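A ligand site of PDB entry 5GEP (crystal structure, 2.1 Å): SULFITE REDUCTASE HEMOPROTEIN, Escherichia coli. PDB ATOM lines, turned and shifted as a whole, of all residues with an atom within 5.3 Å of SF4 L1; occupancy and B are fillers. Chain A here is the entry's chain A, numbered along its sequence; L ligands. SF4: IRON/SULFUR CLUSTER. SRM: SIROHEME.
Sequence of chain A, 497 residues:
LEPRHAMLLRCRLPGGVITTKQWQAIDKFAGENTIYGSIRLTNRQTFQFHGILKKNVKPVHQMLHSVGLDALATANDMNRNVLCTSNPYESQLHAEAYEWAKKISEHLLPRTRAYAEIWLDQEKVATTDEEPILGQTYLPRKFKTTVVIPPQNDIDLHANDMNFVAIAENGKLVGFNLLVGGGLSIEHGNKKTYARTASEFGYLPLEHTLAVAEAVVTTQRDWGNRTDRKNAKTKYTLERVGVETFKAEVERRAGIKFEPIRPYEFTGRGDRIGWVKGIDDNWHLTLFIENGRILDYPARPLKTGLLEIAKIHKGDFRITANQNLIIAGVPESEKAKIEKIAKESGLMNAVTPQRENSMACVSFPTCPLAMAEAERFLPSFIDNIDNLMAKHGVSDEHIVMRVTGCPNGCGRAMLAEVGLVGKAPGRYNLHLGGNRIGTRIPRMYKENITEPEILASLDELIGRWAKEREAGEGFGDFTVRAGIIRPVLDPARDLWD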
ATOM      1  N   CYS A 361     -21.882   5.435   5.991  1.00  0.00           N
ATOM      2  CA  CYS A 361     -21.184   5.647   7.266  1.00  0.00           C
ATOM      3  C   CYS A 361     -21.982   6.673   8.077  1.00  0.00           C
ATOM      4  O   CYS A 361     -22.921   7.281   7.577  1.00  0.00           O
ATOM      5  CB  CYS A 361     -19.771   6.216   7.050  1.00  0.00           C
ATOM      6  SG  CYS A 361     -19.735   7.878   6.295  1.00  0.00           S
ATOM      7  N   VAL A 362     -21.562   6.894   9.317  1.00  0.00           N
ATOM      8  CA  VAL A 362     -22.203   7.872  10.184  1.00  0.00           C
ATOM      9  C   VAL A 362     -22.140   9.292   9.581  1.00  0.00           C
ATOM     10  O   VAL A 362     -23.192   9.930   9.334  1.00  0.00           O
ATOM     11  CB  VAL A 362     -21.569   7.867  11.555  1.00  0.00           C
ATOM     12  CG1 VAL A 362     -22.190   8.948  12.414  1.00  0.00           C
ATOM     13  CG2 VAL A 362     -21.746   6.505  12.201  1.00  0.00           C
ATOM     14  N   SER A 363     -20.926   9.784   9.336  1.00  0.00           N
ATOM     15  CA  SER A 363     -20.748  11.122   8.749  1.00  0.00           C
ATOM     16  C   SER A 363     -21.383  12.175   9.658  1.00  0.00           C
ATOM     17  O   SER A 363     -21.312  12.070  10.874  1.00  0.00           O
ATOM     18  CB  SER A 363     -21.360  11.150   7.358  1.00  0.00           C
ATOM     19  OG  SER A 363     -21.162  12.399   6.729  1.00  0.00           O
ATOM     20  N   CYS A 367     -19.475  13.121  12.846  1.00  0.00           N
ATOM     21  CA  CYS A 367     -18.097  12.913  12.409  1.00  0.00           C
ATOM     22  C   CYS A 367     -17.384  14.228  12.084  1.00  0.00           C
ATOM     23  O   CYS A 367     -17.869  15.012  11.282  1.00  0.00           O
ATOM     24  CB  CYS A 367     -18.024  12.010  11.193  1.00  0.00           C
ATOM     25  SG  CYS A 367     -16.309  11.537  10.834  1.00  0.00           S
ATOM     26  N   LEU A 369     -14.677  14.551  10.411  1.00  0.00           N
ATOM     27  CA  LEU A 369     -14.032  14.435   9.128  1.00  0.00           C
ATOM     28  C   LEU A 369     -15.003  14.362   7.970  1.00  0.00           C
ATOM     29  O   LEU A 369     -14.592  14.307   6.832  1.00  0.00           O
ATOM     30  CB  LEU A 369     -13.162  13.175   9.120  1.00  0.00           C
ATOM     31  CG  LEU A 369     -12.377  12.880  10.391  1.00  0.00           C
ATOM     32  CD1 LEU A 369     -11.577  11.605  10.164  1.00  0.00           C
ATOM     33  CD2 LEU A 369     -11.431  14.040  10.738  1.00  0.00           C
ATOM     34  N   ALA A 370     -16.291  14.357   8.269  1.00  0.00           N
ATOM     35  CA  ALA A 370     -17.302  14.269   7.212  1.00  0.00           C
ATOM     36  C   ALA A 370     -17.232  15.401   6.191  1.00  0.00           C
ATOM     37  O   ALA A 370     -17.131  16.579   6.571  1.00  0.00           O
ATOM     38  CB  ALA A 370     -18.666  14.229   7.842  1.00  0.00           C
ATOM     39  N   MET A 371     -17.279  15.056   4.902  1.00  0.00           N
ATOM     40  CA  MET A 371     -17.234  16.033   3.827  1.00  0.00           C
ATOM     41  C   MET A 371     -18.641  16.197   3.222  1.00  0.00           C
ATOM     42  O   MET A 371     -19.028  17.283   2.787  1.00  0.00           O
ATOM     43  CB  MET A 371     -16.249  15.602   2.740  1.00  0.00           C
ATOM     44  CG  MET A 371     -14.776  15.576   3.167  1.00  0.00           C
ATOM     45  SD  MET A 371     -13.685  15.083   1.816  1.00  0.00           S
ATOM     46  CE  MET A 371     -12.093  15.136   2.584  1.00  0.00           C
ATOM     47  N   ALA A 372     -19.398  15.102   3.204  1.00  0.00           N
ATOM     48  CA  ALA A 372     -20.739  15.107   2.674  1.00  0.00           C
ATOM     49  C   ALA A 372     -21.569  14.168   3.542  1.00  0.00           C
ATOM     50  O   ALA A 372     -20.996  13.319   4.240  1.00  0.00           O
ATOM     51  CB  ALA A 372     -20.740  14.617   1.270  1.00  0.00           C
ATOM     52  N   THR A 404     -20.099   6.754   1.347  1.00  0.00           N
ATOM     53  CA  THR A 404     -19.157   7.080   2.412  1.00  0.00           C
ATOM     54  C   THR A 404     -19.025   8.622   2.432  1.00  0.00           C
ATOM     55  O   THR A 404     -19.052   9.263   1.379  1.00  0.00           O
ATOM     56  CB  THR A 404     -17.805   6.329   2.231  1.00  0.00           C
ATOM     57  OG1 THR A 404     -17.147   6.269   3.480  1.00  0.00           O
ATOM     58  CG2 THR A 404     -16.900   6.985   1.195  1.00  0.00           C
ATOM     59  N   GLY A 405     -18.982   9.184   3.627  1.00  0.00           N
ATOM     60  CA  GLY A 405     -18.917  10.633   3.796  1.00  0.00           C
ATOM     61  C   GLY A 405     -17.638  11.363   3.456  1.00  0.00           C
ATOM     62  O   GLY A 405     -17.652  12.590   3.270  1.00  0.00           O
ATOM     63  N   CYS A 406     -16.530  10.636   3.350  1.00  0.00           N
ATOM     64  CA  CYS A 406     -15.253  11.233   2.996  1.00  0.00           C
ATOM     65  C   CYS A 406     -14.381  10.071   2.521  1.00  0.00           C
ATOM     66  O   CYS A 406     -14.737   8.912   2.705  1.00  0.00           O
ATOM     67  CB  CYS A 406     -14.666  11.998   4.219  1.00  0.00           C
ATOM     68  SG  CYS A 406     -13.875  11.013   5.521  1.00  0.00           S
ATOM     69  N   ASN A 408     -11.953   8.559   3.684  1.00  0.00           N
ATOM     70  CA  ASN A 408     -11.511   7.613   4.692  1.00  0.00           C
ATOM     71  C   ASN A 408     -12.181   6.243   4.395  1.00  0.00           C
ATOM     72  O   ASN A 408     -11.570   5.192   4.588  1.00  0.00           O
ATOM     73  CB  ASN A 408     -11.782   8.120   6.111  1.00  0.00           C
ATOM     74  CG  ASN A 408     -10.715   9.136   6.593  1.00  0.00           C
ATOM     75  OD1 ASN A 408      -9.578   9.143   6.095  1.00  0.00           O
ATOM     76  ND2 ASN A 408     -11.074   9.978   7.571  1.00  0.00           N
ATOM     77  N   GLY A 409     -13.409   6.290   3.895  1.00  0.00           N
ATOM     78  CA  GLY A 409     -14.102   5.080   3.472  1.00  0.00           C
ATOM     79  C   GLY A 409     -14.837   4.169   4.419  1.00  0.00           C
ATOM     80  O   GLY A 409     -15.125   3.020   4.052  1.00  0.00           O
ATOM     81  N   CYS A 410     -15.206   4.653   5.588  1.00  0.00           N
ATOM     82  CA  CYS A 410     -15.912   3.861   6.578  1.00  0.00           C
ATOM     83  C   CYS A 410     -17.182   3.131   6.057  1.00  0.00           C
ATOM     84  O   CYS A 410     -17.506   2.040   6.523  1.00  0.00           O
ATOM     85  CB  CYS A 410     -16.249   4.755   7.768  1.00  0.00           C
ATOM     86  SG  CYS A 410     -14.788   5.562   8.498  1.00  0.00           S
ATOM     87  N   GLY A 411     -17.839   3.703   5.062  1.00  0.00           N
ATOM     88  CA  GLY A 411     -19.044   3.121   4.504  1.00  0.00           C
ATOM     89  C   GLY A 411     -18.769   2.008   3.519  1.00  0.00           C
ATOM     90  O   GLY A 411     -19.716   1.426   2.968  1.00  0.00           O
HETATM   91 FE1  SF4 L   1     -17.807   8.666   7.167  1.00  0.00          FE
HETATM   92 FE2  SF4 L   1     -16.569  10.129   9.079  1.00  0.00          FE
HETATM   93 FE3  SF4 L   1     -15.363   9.933   6.815  1.00  0.00          FE
HETATM   94 FE4  SF4 L   1     -15.714   7.643   8.258  1.00  0.00          FE
HETATM   95  S1  SF4 L   1     -14.462   9.452   8.779  1.00  0.00           S
HETATM   96  S2  SF4 L   1     -15.990   7.906   6.109  1.00  0.00           S
HETATM   97  S3  SF4 L   1     -17.733   8.105   9.202  1.00  0.00           S
HETATM   98  S4  SF4 L   1     -17.380  10.865   7.201  1.00  0.00           S
HETATM   99 FE   SRM L   2     -14.109   4.568  10.382  1.00  0.00          FE
HETATM  100  CHA SRM L   2     -12.375   7.313  11.270  1.00  0.00           C
HETATM  101  CHB SRM L   2     -17.080   5.607  12.086  1.00  0.00           C
HETATM  102  CHC SRM L   2     -15.560   1.476   9.900  1.00  0.00           C
HETATM  103  CHD SRM L   2     -11.827   3.810   7.855  1.00  0.00           C
HETATM  104  NA  SRM L   2     -14.650   6.286  11.637  1.00  0.00           N
HETATM  105  C1A SRM L   2     -13.595   7.289  11.919  1.00  0.00           C
HETATM  106  C2A SRM L   2     -14.340   7.809  13.074  1.00  0.00           C
HETATM  107  CMA SRM L   2     -14.234   6.921  14.249  1.00  0.00           C
HETATM  108  CDA SRM L   2     -14.063   9.356  12.962  1.00  0.00           C
HETATM  109  CEA SRM L   2     -12.824   9.816  13.726  1.00  0.00           C
HETATM  110  O3A SRM L   2     -11.707   9.450  13.349  1.00  0.00           O
HETATM  111  O4A SRM L   2     -12.970  10.525  14.738  1.00  0.00           O
HETATM  112  C3A SRM L   2     -15.618   7.843  12.274  1.00  0.00           C
HETATM  113  CAA SRM L   2     -16.651   8.197  13.410  1.00  0.00           C
HETATM  114  CBA SRM L   2     -17.974   8.798  12.986  1.00  0.00           C
HETATM  115  CCA SRM L   2     -18.956   8.967  14.136  1.00  0.00           C
HETATM  116  O1A SRM L   2     -19.304  10.108  14.473  1.00  0.00           O
HETATM  117  O2A SRM L   2     -19.394   7.955  14.716  1.00  0.00           O
HETATM  118  C4A SRM L   2     -16.038   6.462  12.233  1.00  0.00           C
HETATM  119  NB  SRM L   2     -16.019   3.792  10.710  1.00  0.00           N
HETATM  120  C1B SRM L   2     -17.038   4.417  11.392  1.00  0.00           C
HETATM  121  C2B SRM L   2     -18.239   3.529  11.406  1.00  0.00           C
HETATM  122  CMB SRM L   2     -18.998   3.816  12.726  1.00  0.00           C
HETATM  123  CDB SRM L   2     -18.976   3.576  10.008  1.00  0.00           C
HETATM  124  CEB SRM L   2     -20.410   3.142  10.188  1.00  0.00           C
HETATM  125  O3B SRM L   2     -21.334   3.939   9.954  1.00  0.00           O
HETATM  126  O4B SRM L   2     -20.619   1.993  10.610  1.00  0.00           O
HETATM  127  C3B SRM L   2     -17.408   2.253  11.539  1.00  0.00           C
HETATM  128  CAB SRM L   2     -16.924   1.998  12.936  1.00  0.00           C
HETATM  129  CBB SRM L   2     -16.288   0.634  12.939  1.00  0.00           C
HETATM  130  CCB SRM L   2     -15.942   0.159  14.322  1.00  0.00           C
HETATM  131  O1B SRM L   2     -16.866  -0.234  15.045  1.00  0.00           O
HETATM  132  O2B SRM L   2     -14.746   0.164  14.694  1.00  0.00           O
HETATM  133  C4B SRM L   2     -16.230   2.405  10.615  1.00  0.00           C
HETATM  134  NC  SRM L   2     -13.872   2.963   9.064  1.00  0.00           N
HETATM  135  C1C SRM L   2     -14.446   1.715   9.129  1.00  0.00           C
HETATM  136  C2C SRM L   2     -14.276   1.181   7.791  1.00  0.00           C
HETATM  137  CDC SRM L   2     -14.868  -0.136   7.314  1.00  0.00           C
HETATM  138  CEC SRM L   2     -14.575  -1.362   8.177  1.00  0.00           C
HETATM  139  O3C SRM L   2     -13.711  -1.308   9.066  1.00  0.00           O
HETATM  140  O4C SRM L   2     -15.231  -2.382   7.969  1.00  0.00           O
HETATM  141  C3C SRM L   2     -13.123   1.766   7.289  1.00  0.00           C
HETATM  142  CAC SRM L   2     -12.498   1.548   5.933  1.00  0.00           C
HETATM  143  CBC SRM L   2     -11.544   0.348   5.836  1.00  0.00           C
HETATM  144  CCC SRM L   2     -10.134   0.682   6.224  1.00  0.00           C
HETATM  145  O1C SRM L   2      -9.828   0.749   7.412  1.00  0.00           O
HETATM  146  O2C SRM L   2      -9.309   0.847   5.346  1.00  0.00           O
HETATM  147  C4C SRM L   2     -12.922   2.964   8.039  1.00  0.00           C
HETATM  148  ND  SRM L   2     -12.267   5.340   9.725  1.00  0.00           N
HETATM  149  C1D SRM L   2     -11.559   4.917   8.652  1.00  0.00           C
HETATM  150  C2D SRM L   2     -10.469   5.850   8.711  1.00  0.00           C
HETATM  151  CAD SRM L   2      -9.345   5.660   7.748  1.00  0.00           C
HETATM  152  CBD SRM L   2      -8.199   4.920   8.411  1.00  0.00           C
HETATM  153  CCD SRM L   2      -6.971   4.821   7.529  1.00  0.00           C
HETATM  154  O1D SRM L   2      -6.331   3.747   7.561  1.00  0.00           O
HETATM  155  O2D SRM L   2      -6.630   5.784   6.830  1.00  0.00           O
HETATM  156  C3D SRM L   2     -10.571   6.748   9.777  1.00  0.00           C
HETATM  157  CDD SRM L   2      -9.910   8.056  10.063  1.00  0.00           C
HETATM  158  CED SRM L   2      -8.623   7.783  10.786  1.00  0.00           C
HETATM  159  O3D SRM L   2      -8.614   6.983  11.755  1.00  0.00           O
HETATM  160  O4D SRM L   2      -7.602   8.367  10.376  1.00  0.00           O
HETATM  161  C4D SRM L   2     -11.764   6.406  10.436  1.00  0.00           C
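FE3 of SF4 L1 is bound by SG of Cys 406, 2.2 Å away. SG of Cys 361 binds FE1 of SF4 L1, at 2.3 Å. An iron atom (FE2) of SF4 L1 is bound by the side-chain sulfur of Cys 367 (2.3 Å). The backbone NH (N) of Cys 410 sits close to a sulfur (S2) of SF4 L1, at 3.4 Å. FE4 of SF4 L1 is bound by SG of Cys 410, at 2.3 Å. OG1 of Thr 404 lies close to S2 of SF4 L1 (3.3 Å). The backbone NH (N) of Ser 363 sits close to a sulfur (S3) of SF4 L1, 3.6 Å away. The side-chain amide nitrogen of Asn 408 sits close to a sulfur (S1) of SF4 L1, 3.6 Å away. The backbone NH of Gly 409 lies close to a sulfur (S2) of SF4 L1 (3.8 Å). An oxygen (O1A) of SRM L2 lies within hydrogen-bond range of the backbone NH (N) of Cys 367, at 3.4 Å. An iron atom (FE) of SRM L2 is bound by the side-chain sulfur (SG) of Cys 410 (2.2 Å). O3B of SRM L2 lies within hydrogen-bond range of N of Val 362.
N of Asn 408 lies close to SG of Cys 406 (3.6 Å). O of Leu 369 lies close to SG of Cys 406, 3.6 Å away. N of Gly 405 lies close to SG of Cys 361 (3.1 Å). The side-chain sulfur (SG) of Cys 367 sits close to the backbone NH (N) of Leu 369, 3.5 Å away. The backbone NH (N) of Cys 410 lies within hydrogen-bond range of the side-chain hydroxyl (OG1) of Thr 404 (3.3 Å). OG1 of Thr 404 lies within hydrogen-bond range of N of Gly 411. The side-chain hydroxyl (OG) of Ser 363 is in hydrogen-bond range of the backbone carbonyl oxygen (O) of Ala 372. O of Gly 405 lies within hydrogen-bond range of N of Met 371 (3.0 Å).
Residues that only touch SF4 L1: Leu 369 (3.9 Å), Ala 370 (3.4 Å) and Gly 405 (3.7 Å). Hydrophobic or aromatic side chains that line SF4 L1: Leu 369 and Ala 370. Within 4 Å of SF4 L1: Cys 361, Ser 363, Cys 367, Leu 369, Ala 370, Thr 404, Gly 405, Cys 406, Asn 408, Gly 409 and Cys 410.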
